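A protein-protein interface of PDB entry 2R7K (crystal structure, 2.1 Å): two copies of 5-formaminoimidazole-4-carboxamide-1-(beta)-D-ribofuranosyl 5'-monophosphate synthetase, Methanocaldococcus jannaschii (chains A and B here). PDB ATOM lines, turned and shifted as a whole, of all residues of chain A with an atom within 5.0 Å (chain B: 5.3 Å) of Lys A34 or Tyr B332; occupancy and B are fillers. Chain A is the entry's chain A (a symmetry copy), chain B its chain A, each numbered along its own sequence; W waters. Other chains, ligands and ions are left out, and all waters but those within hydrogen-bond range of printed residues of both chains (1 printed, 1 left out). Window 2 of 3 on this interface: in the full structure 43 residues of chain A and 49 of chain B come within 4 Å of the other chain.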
ATOM      1  N   SER A  29      34.625   5.138 -32.234  1.00  0.00           N
ATOM      2  CA  SER A  29      34.261   6.106 -31.208  1.00  0.00           C
ATOM      3  C   SER A  29      33.512   5.492 -30.017  1.00  0.00           C
ATOM      4  O   SER A  29      33.588   6.005 -28.903  1.00  0.00           O
ATOM      5  CB  SER A  29      33.469   7.266 -31.812  1.00  0.00           C
ATOM      6  OG  SER A  29      32.172   6.846 -32.180  1.00  0.00           O
ATOM      7  N   LEU A  30      32.801   4.393 -30.241  1.00  0.00           N
ATOM      8  CA  LEU A  30      32.016   3.784 -29.164  1.00  0.00           C
ATOM      9  C   LEU A  30      32.844   3.430 -27.940  1.00  0.00           C
ATOM     10  O   LEU A  30      32.431   3.726 -26.827  1.00  0.00           O
ATOM     11  CB  LEU A  30      31.234   2.570 -29.646  1.00  0.00           C
ATOM     12  CG  LEU A  30      30.001   2.896 -30.479  1.00  0.00           C
ATOM     13  CD1 LEU A  30      29.334   1.615 -30.945  1.00  0.00           C
ATOM     14  CD2 LEU A  30      29.035   3.758 -29.686  1.00  0.00           C
ATOM     15  N   HIS A  31      34.004   2.808 -28.135  1.00  0.00           N
ATOM     16  CA  HIS A  31      34.872   2.483 -26.999  1.00  0.00           C
ATOM     17  C   HIS A  31      35.880   3.570 -26.649  1.00  0.00           C
ATOM     18  O   HIS A  31      36.395   3.603 -25.536  1.00  0.00           O
ATOM     19  CB  HIS A  31      35.554   1.120 -27.159  1.00  0.00           C
ATOM     20  CG  HIS A  31      36.467   1.017 -28.339  1.00  0.00           C
ATOM     21  ND1 HIS A  31      37.807   1.328 -28.270  1.00  0.00           N
ATOM     22  CD2 HIS A  31      36.243   0.591 -29.605  1.00  0.00           C
ATOM     23  CE1 HIS A  31      38.367   1.116 -29.446  1.00  0.00           C
ATOM     24  NE2 HIS A  31      37.442   0.659 -30.271  1.00  0.00           N
ATOM     25  N   ILE A  32      36.164   4.457 -27.596  1.00  0.00           N
ATOM     26  CA  ILE A  32      36.900   5.670 -27.281  1.00  0.00           C
ATOM     27  C   ILE A  32      36.105   6.473 -26.251  1.00  0.00           C
ATOM     28  O   ILE A  32      36.661   6.969 -25.274  1.00  0.00           O
ATOM     29  CB  ILE A  32      37.117   6.554 -28.534  1.00  0.00           C
ATOM     30  CG1 ILE A  32      38.196   5.954 -29.439  1.00  0.00           C
ATOM     31  CG2 ILE A  32      37.469   7.990 -28.130  1.00  0.00           C
ATOM     32  CD1 ILE A  32      38.328   6.662 -30.801  1.00  0.00           C
ATOM     33  N   LEU A  33      34.801   6.589 -26.481  1.00  0.00           N
ATOM     34  CA  LEU A  33      33.934   7.376 -25.614  1.00  0.00           C
ATOM     35  C   LEU A  33      33.573   6.621 -24.334  1.00  0.00           C
ATOM     36  O   LEU A  33      33.670   7.174 -23.237  1.00  0.00           O
ATOM     37  CB  LEU A  33      32.678   7.825 -26.364  1.00  0.00           C
ATOM     38  CG  LEU A  33      32.933   8.777 -27.539  1.00  0.00           C
ATOM     39  CD1 LEU A  33      31.630   9.148 -28.218  1.00  0.00           C
ATOM     40  CD2 LEU A  33      33.693  10.029 -27.100  1.00  0.00           C
ATOM     41  N   LYS A  34      33.173   5.361 -24.474  1.00  0.00           N
ATOM     42  CA  LYS A  34      32.913   4.516 -23.308  1.00  0.00           C
ATOM     43  C   LYS A  34      34.150   4.411 -22.418  1.00  0.00           C
ATOM     44  O   LYS A  34      34.064   4.540 -21.197  1.00  0.00           O
ATOM     45  CB  LYS A  34      32.444   3.124 -23.726  1.00  0.00           C
ATOM     46  CG  LYS A  34      32.081   2.192 -22.553  1.00  0.00           C
ATOM     47  CD  LYS A  34      30.885   2.715 -21.786  1.00  0.00           C
ATOM     48  CE  LYS A  34      30.584   1.862 -20.557  1.00  0.00           C
ATOM     49  NZ  LYS A  34      29.315   2.286 -19.922  1.00  0.00           N
ATOM     50  N   GLY A  35      35.300   4.183 -23.031  1.00  0.00           N
ATOM     51  CA  GLY A  35      36.554   4.077 -22.285  1.00  0.00           C
ATOM     52  C   GLY A  35      36.858   5.334 -21.497  1.00  0.00           C
ATOM     53  O   GLY A  35      37.351   5.273 -20.368  1.00  0.00           O
ATOM     54  N   ALA A  36      36.570   6.480 -22.109  1.00  0.00           N
ATOM     55  CA  ALA A  36      36.750   7.776 -21.474  1.00  0.00           C
ATOM     56  C   ALA A  36      35.861   7.926 -20.239  1.00  0.00           C
ATOM     57  O   ALA A  36      36.332   8.320 -19.183  1.00  0.00           O
ATOM     58  CB  ALA A  36      36.457   8.886 -22.466  1.00  0.00           C
ATOM     59  N   LYS A  37      34.575   7.624 -20.392  1.00  0.00           N
ATOM     60  CA  LYS A  37      33.635   7.657 -19.287  1.00  0.00           C
ATOM     61  C   LYS A  37      34.096   6.758 -18.148  1.00  0.00           C
ATOM     62  O   LYS A  37      34.040   7.152 -16.987  1.00  0.00           O
ATOM     63  CB  LYS A  37      32.240   7.228 -19.752  1.00  0.00           C
ATOM     64  CG  LYS A  37      31.573   8.201 -20.701  1.00  0.00           C
ATOM     65  CD  LYS A  37      30.774   9.243 -19.970  1.00  0.00           C
ATOM     66  CE  LYS A  37      29.435   8.689 -19.533  1.00  0.00           C
ATOM     67  NZ  LYS A  37      28.628   9.725 -18.842  1.00  0.00           N
ATOM     68  N   LEU A  38      34.550   5.552 -18.486  1.00  0.00           N
ATOM     69  CA  LEU A  38      35.005   4.582 -17.486  1.00  0.00           C
ATOM     70  C   LEU A  38      36.227   5.106 -16.729  1.00  0.00           C
ATOM     71  O   LEU A  38      36.473   4.718 -15.585  1.00  0.00           O
ATOM     72  CB  LEU A  38      35.332   3.223 -18.137  1.00  0.00           C
ATOM     73  CG  LEU A  38      34.146   2.343 -18.549  1.00  0.00           C
ATOM     74  CD1 LEU A  38      34.615   1.174 -19.401  1.00  0.00           C
ATOM     75  CD2 LEU A  38      33.393   1.825 -17.322  1.00  0.00           C
ATOM     76  N   ARG A  57      21.855   5.826 -27.927  1.00  0.00           N
ATOM     77  CA  ARG A  57      21.279   4.643 -27.310  1.00  0.00           C
ATOM     78  C   ARG A  57      22.306   3.881 -26.479  1.00  0.00           C
ATOM     79  O   ARG A  57      21.947   3.186 -25.538  1.00  0.00           O
ATOM     80  CB  ARG A  57      20.623   3.735 -28.353  1.00  0.00           C
ATOM     81  CG  ARG A  57      19.625   4.462 -29.240  1.00  0.00           C
ATOM     82  CD  ARG A  57      18.310   3.712 -29.362  1.00  0.00           C
ATOM     83  NE  ARG A  57      17.395   4.416 -30.255  1.00  0.00           N
ATOM     84  CZ  ARG A  57      16.774   3.868 -31.295  1.00  0.00           C
ATOM     85  NH1 ARG A  57      16.923   2.581 -31.571  1.00  0.00           N
ATOM     86  NH2 ARG A  57      15.979   4.613 -32.052  1.00  0.00           N
ATOM     87  N   PHE A  58      23.578   4.010 -26.827  1.00  0.00           N
ATOM     88  CA  PHE A  58      24.628   3.369 -26.038  1.00  0.00           C
ATOM     89  C   PHE A  58      25.086   4.294 -24.902  1.00  0.00           C
ATOM     90  O   PHE A  58      25.835   3.879 -24.025  1.00  0.00           O
ATOM     91  CB  PHE A  58      25.817   2.963 -26.916  1.00  0.00           C
ATOM     92  CG  PHE A  58      25.614   1.670 -27.675  1.00  0.00           C
ATOM     93  CD1 PHE A  58      25.253   0.508 -27.013  1.00  0.00           C
ATOM     94  CD2 PHE A  58      25.821   1.616 -29.045  1.00  0.00           C
ATOM     95  CE1 PHE A  58      25.085  -0.686 -27.706  1.00  0.00           C
ATOM     96  CE2 PHE A  58      25.656   0.425 -29.746  1.00  0.00           C
ATOM     97  CZ  PHE A  58      25.287  -0.725 -29.077  1.00  0.00           C
ATOM     98  N   VAL A  60      27.113   6.928 -24.497  1.00  0.00           N
ATOM     99  CA  VAL A  60      28.548   7.062 -24.281  1.00  0.00           C
ATOM    100  C   VAL A  60      29.017   8.496 -24.405  1.00  0.00           C
ATOM    101  O   VAL A  60      30.188   8.793 -24.160  1.00  0.00           O
ATOM    102  CB  VAL A  60      29.370   6.193 -25.279  1.00  0.00           C
ATOM    103  CG1 VAL A  60      29.178   4.713 -24.999  1.00  0.00           C
ATOM    104  CG2 VAL A  60      29.014   6.531 -26.724  1.00  0.00           C
ATOM    105  N   GLU B 221      17.154  -1.628 -28.753  1.00  0.00           N
ATOM    106  CA  GLU B 221      18.552  -1.697 -28.309  1.00  0.00           C
ATOM    107  C   GLU B 221      19.315  -2.721 -29.139  1.00  0.00           C
ATOM    108  O   GLU B 221      18.744  -3.728 -29.552  1.00  0.00           O
ATOM    109  CB  GLU B 221      18.623  -2.090 -26.823  1.00  0.00           C
ATOM    110  CG  GLU B 221      17.872  -1.139 -25.899  1.00  0.00           C
ATOM    111  CD  GLU B 221      17.596  -1.724 -24.522  1.00  0.00           C
ATOM    112  OE1 GLU B 221      18.117  -2.813 -24.184  1.00  0.00           O
ATOM    113  OE2 GLU B 221      16.845  -1.077 -23.765  1.00  0.00           O
ATOM    114  N   LEU B 222      20.595  -2.457 -29.385  1.00  0.00           N
ATOM    115  CA  LEU B 222      21.484  -3.455 -29.973  1.00  0.00           C
ATOM    116  C   LEU B 222      22.262  -4.186 -28.880  1.00  0.00           C
ATOM    117  O   LEU B 222      23.008  -3.564 -28.106  1.00  0.00           O
ATOM    118  CB  LEU B 222      22.442  -2.806 -30.974  1.00  0.00           C
ATOM    119  CG  LEU B 222      23.575  -3.681 -31.522  1.00  0.00           C
ATOM    120  CD1 LEU B 222      23.039  -4.846 -32.345  1.00  0.00           C
ATOM    121  CD2 LEU B 222      24.519  -2.818 -32.341  1.00  0.00           C
ATOM    122  N   LEU B 223      22.089  -5.506 -28.829  1.00  0.00           N
ATOM    123  CA  LEU B 223      22.688  -6.340 -27.789  1.00  0.00           C
ATOM    124  C   LEU B 223      23.936  -7.100 -28.237  1.00  0.00           C
ATOM    125  O   LEU B 223      24.887  -7.261 -27.466  1.00  0.00           O
ATOM    126  CB  LEU B 223      21.646  -7.305 -27.206  1.00  0.00           C
ATOM    127  CG  LEU B 223      20.870  -6.799 -25.981  1.00  0.00           C
ATOM    128  CD1 LEU B 223      21.815  -6.641 -24.812  1.00  0.00           C
ATOM    129  CD2 LEU B 223      20.156  -5.476 -26.257  1.00  0.00           C
ATOM    130  N   PHE B 272      20.602   0.217 -36.718  1.00  0.00           N
ATOM    131  CA  PHE B 272      19.567   0.712 -35.814  1.00  0.00           C
ATOM    132  C   PHE B 272      18.300   1.086 -36.580  1.00  0.00           C
ATOM    133  O   PHE B 272      17.186   0.785 -36.139  1.00  0.00           O
ATOM    134  CB  PHE B 272      20.082   1.903 -34.999  1.00  0.00           C
ATOM    135  CG  PHE B 272      20.847   1.506 -33.755  1.00  0.00           C
ATOM    136  CD1 PHE B 272      22.226   1.611 -33.710  1.00  0.00           C
ATOM    137  CD2 PHE B 272      20.180   1.024 -32.636  1.00  0.00           C
ATOM    138  CE1 PHE B 272      22.938   1.240 -32.562  1.00  0.00           C
ATOM    139  CE2 PHE B 272      20.879   0.653 -31.489  1.00  0.00           C
ATOM    140  CZ  PHE B 272      22.256   0.768 -31.450  1.00  0.00           C
ATOM    141  N   TYR B 328      28.997  -4.994 -27.678  1.00  0.00           N
ATOM    142  CA  TYR B 328      27.871  -4.056 -27.693  1.00  0.00           C
ATOM    143  C   TYR B 328      27.104  -4.001 -26.363  1.00  0.00           C
ATOM    144  O   TYR B 328      26.785  -2.916 -25.873  1.00  0.00           O
ATOM    145  CB  TYR B 328      26.917  -4.382 -28.856  1.00  0.00           C
ATOM    146  CG  TYR B 328      27.579  -4.214 -30.208  1.00  0.00           C
ATOM    147  CD1 TYR B 328      27.960  -2.957 -30.658  1.00  0.00           C
ATOM    148  CD2 TYR B 328      27.843  -5.315 -31.023  1.00  0.00           C
ATOM    149  CE1 TYR B 328      28.588  -2.788 -31.889  1.00  0.00           C
ATOM    150  CE2 TYR B 328      28.471  -5.159 -32.260  1.00  0.00           C
ATOM    151  CZ  TYR B 328      28.835  -3.899 -32.686  1.00  0.00           C
ATOM    152  OH  TYR B 328      29.452  -3.735 -33.904  1.00  0.00           O
ATOM    153  N   SER B 329      26.815  -5.165 -25.781  1.00  0.00           N
ATOM    154  CA  SER B 329      26.042  -5.225 -24.539  1.00  0.00           C
ATOM    155  C   SER B 329      26.809  -4.585 -23.367  1.00  0.00           C
ATOM    156  O   SER B 329      26.205  -4.056 -22.438  1.00  0.00           O
ATOM    157  CB  SER B 329      25.577  -6.661 -24.227  1.00  0.00           C
ATOM    158  OG  SER B 329      26.617  -7.449 -23.671  1.00  0.00           O
ATOM    159  N   PHE B 330      28.139  -4.603 -23.454  1.00  0.00           N
ATOM    160  CA  PHE B 330      29.029  -3.962 -22.478  1.00  0.00           C
ATOM    161  C   PHE B 330      28.864  -2.448 -22.399  1.00  0.00           C
ATOM    162  O   PHE B 330      29.049  -1.861 -21.333  1.00  0.00           O
ATOM    163  CB  PHE B 330      30.482  -4.263 -22.842  1.00  0.00           C
ATOM    164  CG  PHE B 330      31.501  -3.682 -21.888  1.00  0.00           C
ATOM    165  CD1 PHE B 330      31.803  -4.328 -20.703  1.00  0.00           C
ATOM    166  CD2 PHE B 330      32.197  -2.525 -22.210  1.00  0.00           C
ATOM    167  CE1 PHE B 330      32.758  -3.817 -19.832  1.00  0.00           C
ATOM    168  CE2 PHE B 330      33.149  -2.005 -21.344  1.00  0.00           C
ATOM    169  CZ  PHE B 330      33.423  -2.647 -20.155  1.00  0.00           C
ATOM    170  N   LEU B 331      28.545  -1.806 -23.519  1.00  0.00           N
ATOM    171  CA  LEU B 331      28.602  -0.343 -23.566  1.00  0.00           C
ATOM    172  C   LEU B 331      27.594   0.346 -22.652  1.00  0.00           C
ATOM    173  O   LEU B 331      27.870   1.427 -22.142  1.00  0.00           O
ATOM    174  CB  LEU B 331      28.455   0.181 -25.000  1.00  0.00           C
ATOM    175  CG  LEU B 331      29.513  -0.276 -26.000  1.00  0.00           C
ATOM    176  CD1 LEU B 331      29.084   0.071 -27.409  1.00  0.00           C
ATOM    177  CD2 LEU B 331      30.870   0.347 -25.675  1.00  0.00           C
ATOM    178  N   TYR B 332      26.432  -0.275 -22.456  1.00  0.00           N
ATOM    179  CA  TYR B 332      25.368   0.324 -21.654  1.00  0.00           C
ATOM    180  C   TYR B 332      25.798   0.673 -20.223  1.00  0.00           C
ATOM    181  O   TYR B 332      25.613   1.804 -19.774  1.00  0.00           O
ATOM    182  CB  TYR B 332      24.121  -0.572 -21.638  1.00  0.00           C
ATOM    183  CG  TYR B 332      23.521  -0.760 -23.019  1.00  0.00           C
ATOM    184  CD1 TYR B 332      22.863   0.286 -23.660  1.00  0.00           C
ATOM    185  CD2 TYR B 332      23.644  -1.974 -23.695  1.00  0.00           C
ATOM    186  CE1 TYR B 332      22.325   0.124 -24.927  1.00  0.00           C
ATOM    187  CE2 TYR B 332      23.114  -2.148 -24.968  1.00  0.00           C
ATOM    188  CZ  TYR B 332      22.453  -1.097 -25.576  1.00  0.00           C
ATOM    189  OH  TYR B 332      21.924  -1.259 -26.835  1.00  0.00           O
ATOM    190  N   ASN B 333      26.373  -0.297 -19.518  1.00  0.00           N
ATOM    191  CA  ASN B 333      26.744  -0.114 -18.115  1.00  0.00           C
ATOM    192  C   ASN B 333      28.058  -0.794 -17.757  1.00  0.00           C
ATOM    193  O   ASN B 333      28.334  -1.036 -16.581  1.00  0.00           O
ATOM    194  CB  ASN B 333      25.636  -0.669 -17.214  1.00  0.00           C
ATOM    195  CG  ASN B 333      24.334   0.095 -17.349  1.00  0.00           C
ATOM    196  OD1 ASN B 333      24.282   1.299 -17.107  1.00  0.00           O
ATOM    197  ND2 ASN B 333      23.275  -0.603 -17.738  1.00  0.00           N
ATOM    198  N   GLY B 334      28.856  -1.125 -18.768  1.00  0.00           N
ATOM    199  CA  GLY B 334      30.112  -1.836 -18.558  1.00  0.00           C
ATOM    200  C   GLY B 334      29.951  -3.181 -17.874  1.00  0.00           C
ATOM    201  O   GLY B 334      30.796  -3.591 -17.081  1.00  0.00           O
ATOM    202  N   LEU B 337      26.607  -8.352 -19.934  1.00  0.00           N
ATOM    203  CA  LEU B 337      25.165  -8.535 -20.092  1.00  0.00           C
ATOM    204  C   LEU B 337      24.809  -9.477 -21.250  1.00  0.00           C
ATOM    205  O   LEU B 337      25.133  -9.193 -22.408  1.00  0.00           O
ATOM    206  CB  LEU B 337      24.519  -7.163 -20.329  1.00  0.00           C
ATOM    207  CG  LEU B 337      23.016  -7.030 -20.599  1.00  0.00           C
ATOM    208  CD1 LEU B 337      22.186  -7.293 -19.345  1.00  0.00           C
ATOM    209  CD2 LEU B 337      22.736  -5.636 -21.117  1.00  0.00           C
HETATM  210  O   HOH W   1      29.238   2.152 -17.090  1.00  0.00           O
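Of the printed residues of chain B, Lys A34 touches Leu B331, Tyr B332, Asn B333 and Gly B334. Printed residues of chain A within 4 Å of Leu B331: Leu A30 (3.9 Å), Lys A34 (2.8 Å) and Phe A58 (3.7 Å). Of the printed residues of chain A, Asn B333 touches Lys A34. Printed residues of chain A within 4 Å of Gly B334: Lys A34. Printed residues of chain A within 4 Å of Tyr B328: Phe A58 (3.4 Å). The nearest residue of chain B that does not touch Lys A34 is Phe B330 (4.1 Å).
No position is printed for both chains. Of the 12 pairs that touch across the chains among the printed residues, none has its exchanged pair printed and touching as well.
CD1 of Leu A30 touches CD1 of Leu B331, at 3.9 Å. Lys A34 touches Tyr B332 (NZ to O, 3.7 Å). Gly B334 touches Lys A34 (N to NZ, 3.6 Å). Arg A57 touches Phe B272. Arg A57 touches Tyr B332. Leu B222 touches Phe A58 (O to CE1, 3.6 Å). CE2 of Phe A58 touches CZ of Phe B272, 3.8 Å away. O of Tyr B328 touches CE1 of Phe A58, 3.4 Å away. O of Phe A58 touches O of Leu B331 (3.7 Å). OH of Tyr B332 touches CE1 of Phe A58, 3.3 Å away.
Of the 13 printed residues of chain A, 4 touch a printed residue of chain B. Hydrophobic or aromatic side chains of chain A within 4 Å of the printed part of chain B: Leu A30 and Phe A58. Hydrophobic or aromatic side chains of chain B within 4 Å of the printed part of chain A: Leu B222, Phe B272, Tyr B328, Leu B331 and Tyr B332. Among the printed residues, no Asp or Glu carboxylate lies within 4 Å of a Lys or Arg side-chain nitrogen of the other chain.
OH of Tyr B332 lies within hydrogen-bond range of O of Leu B222, 2.8 Å away.
The side-chain amino group (NZ) of Lys A34 is in hydrogen-bond range of the backbone carbonyl oxygen (O) of Leu B331.
Water W1 lies within hydrogen-bond range of NZ of Lys A34 (2.8 Å) and O of Asn B333 (3.4 Å).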
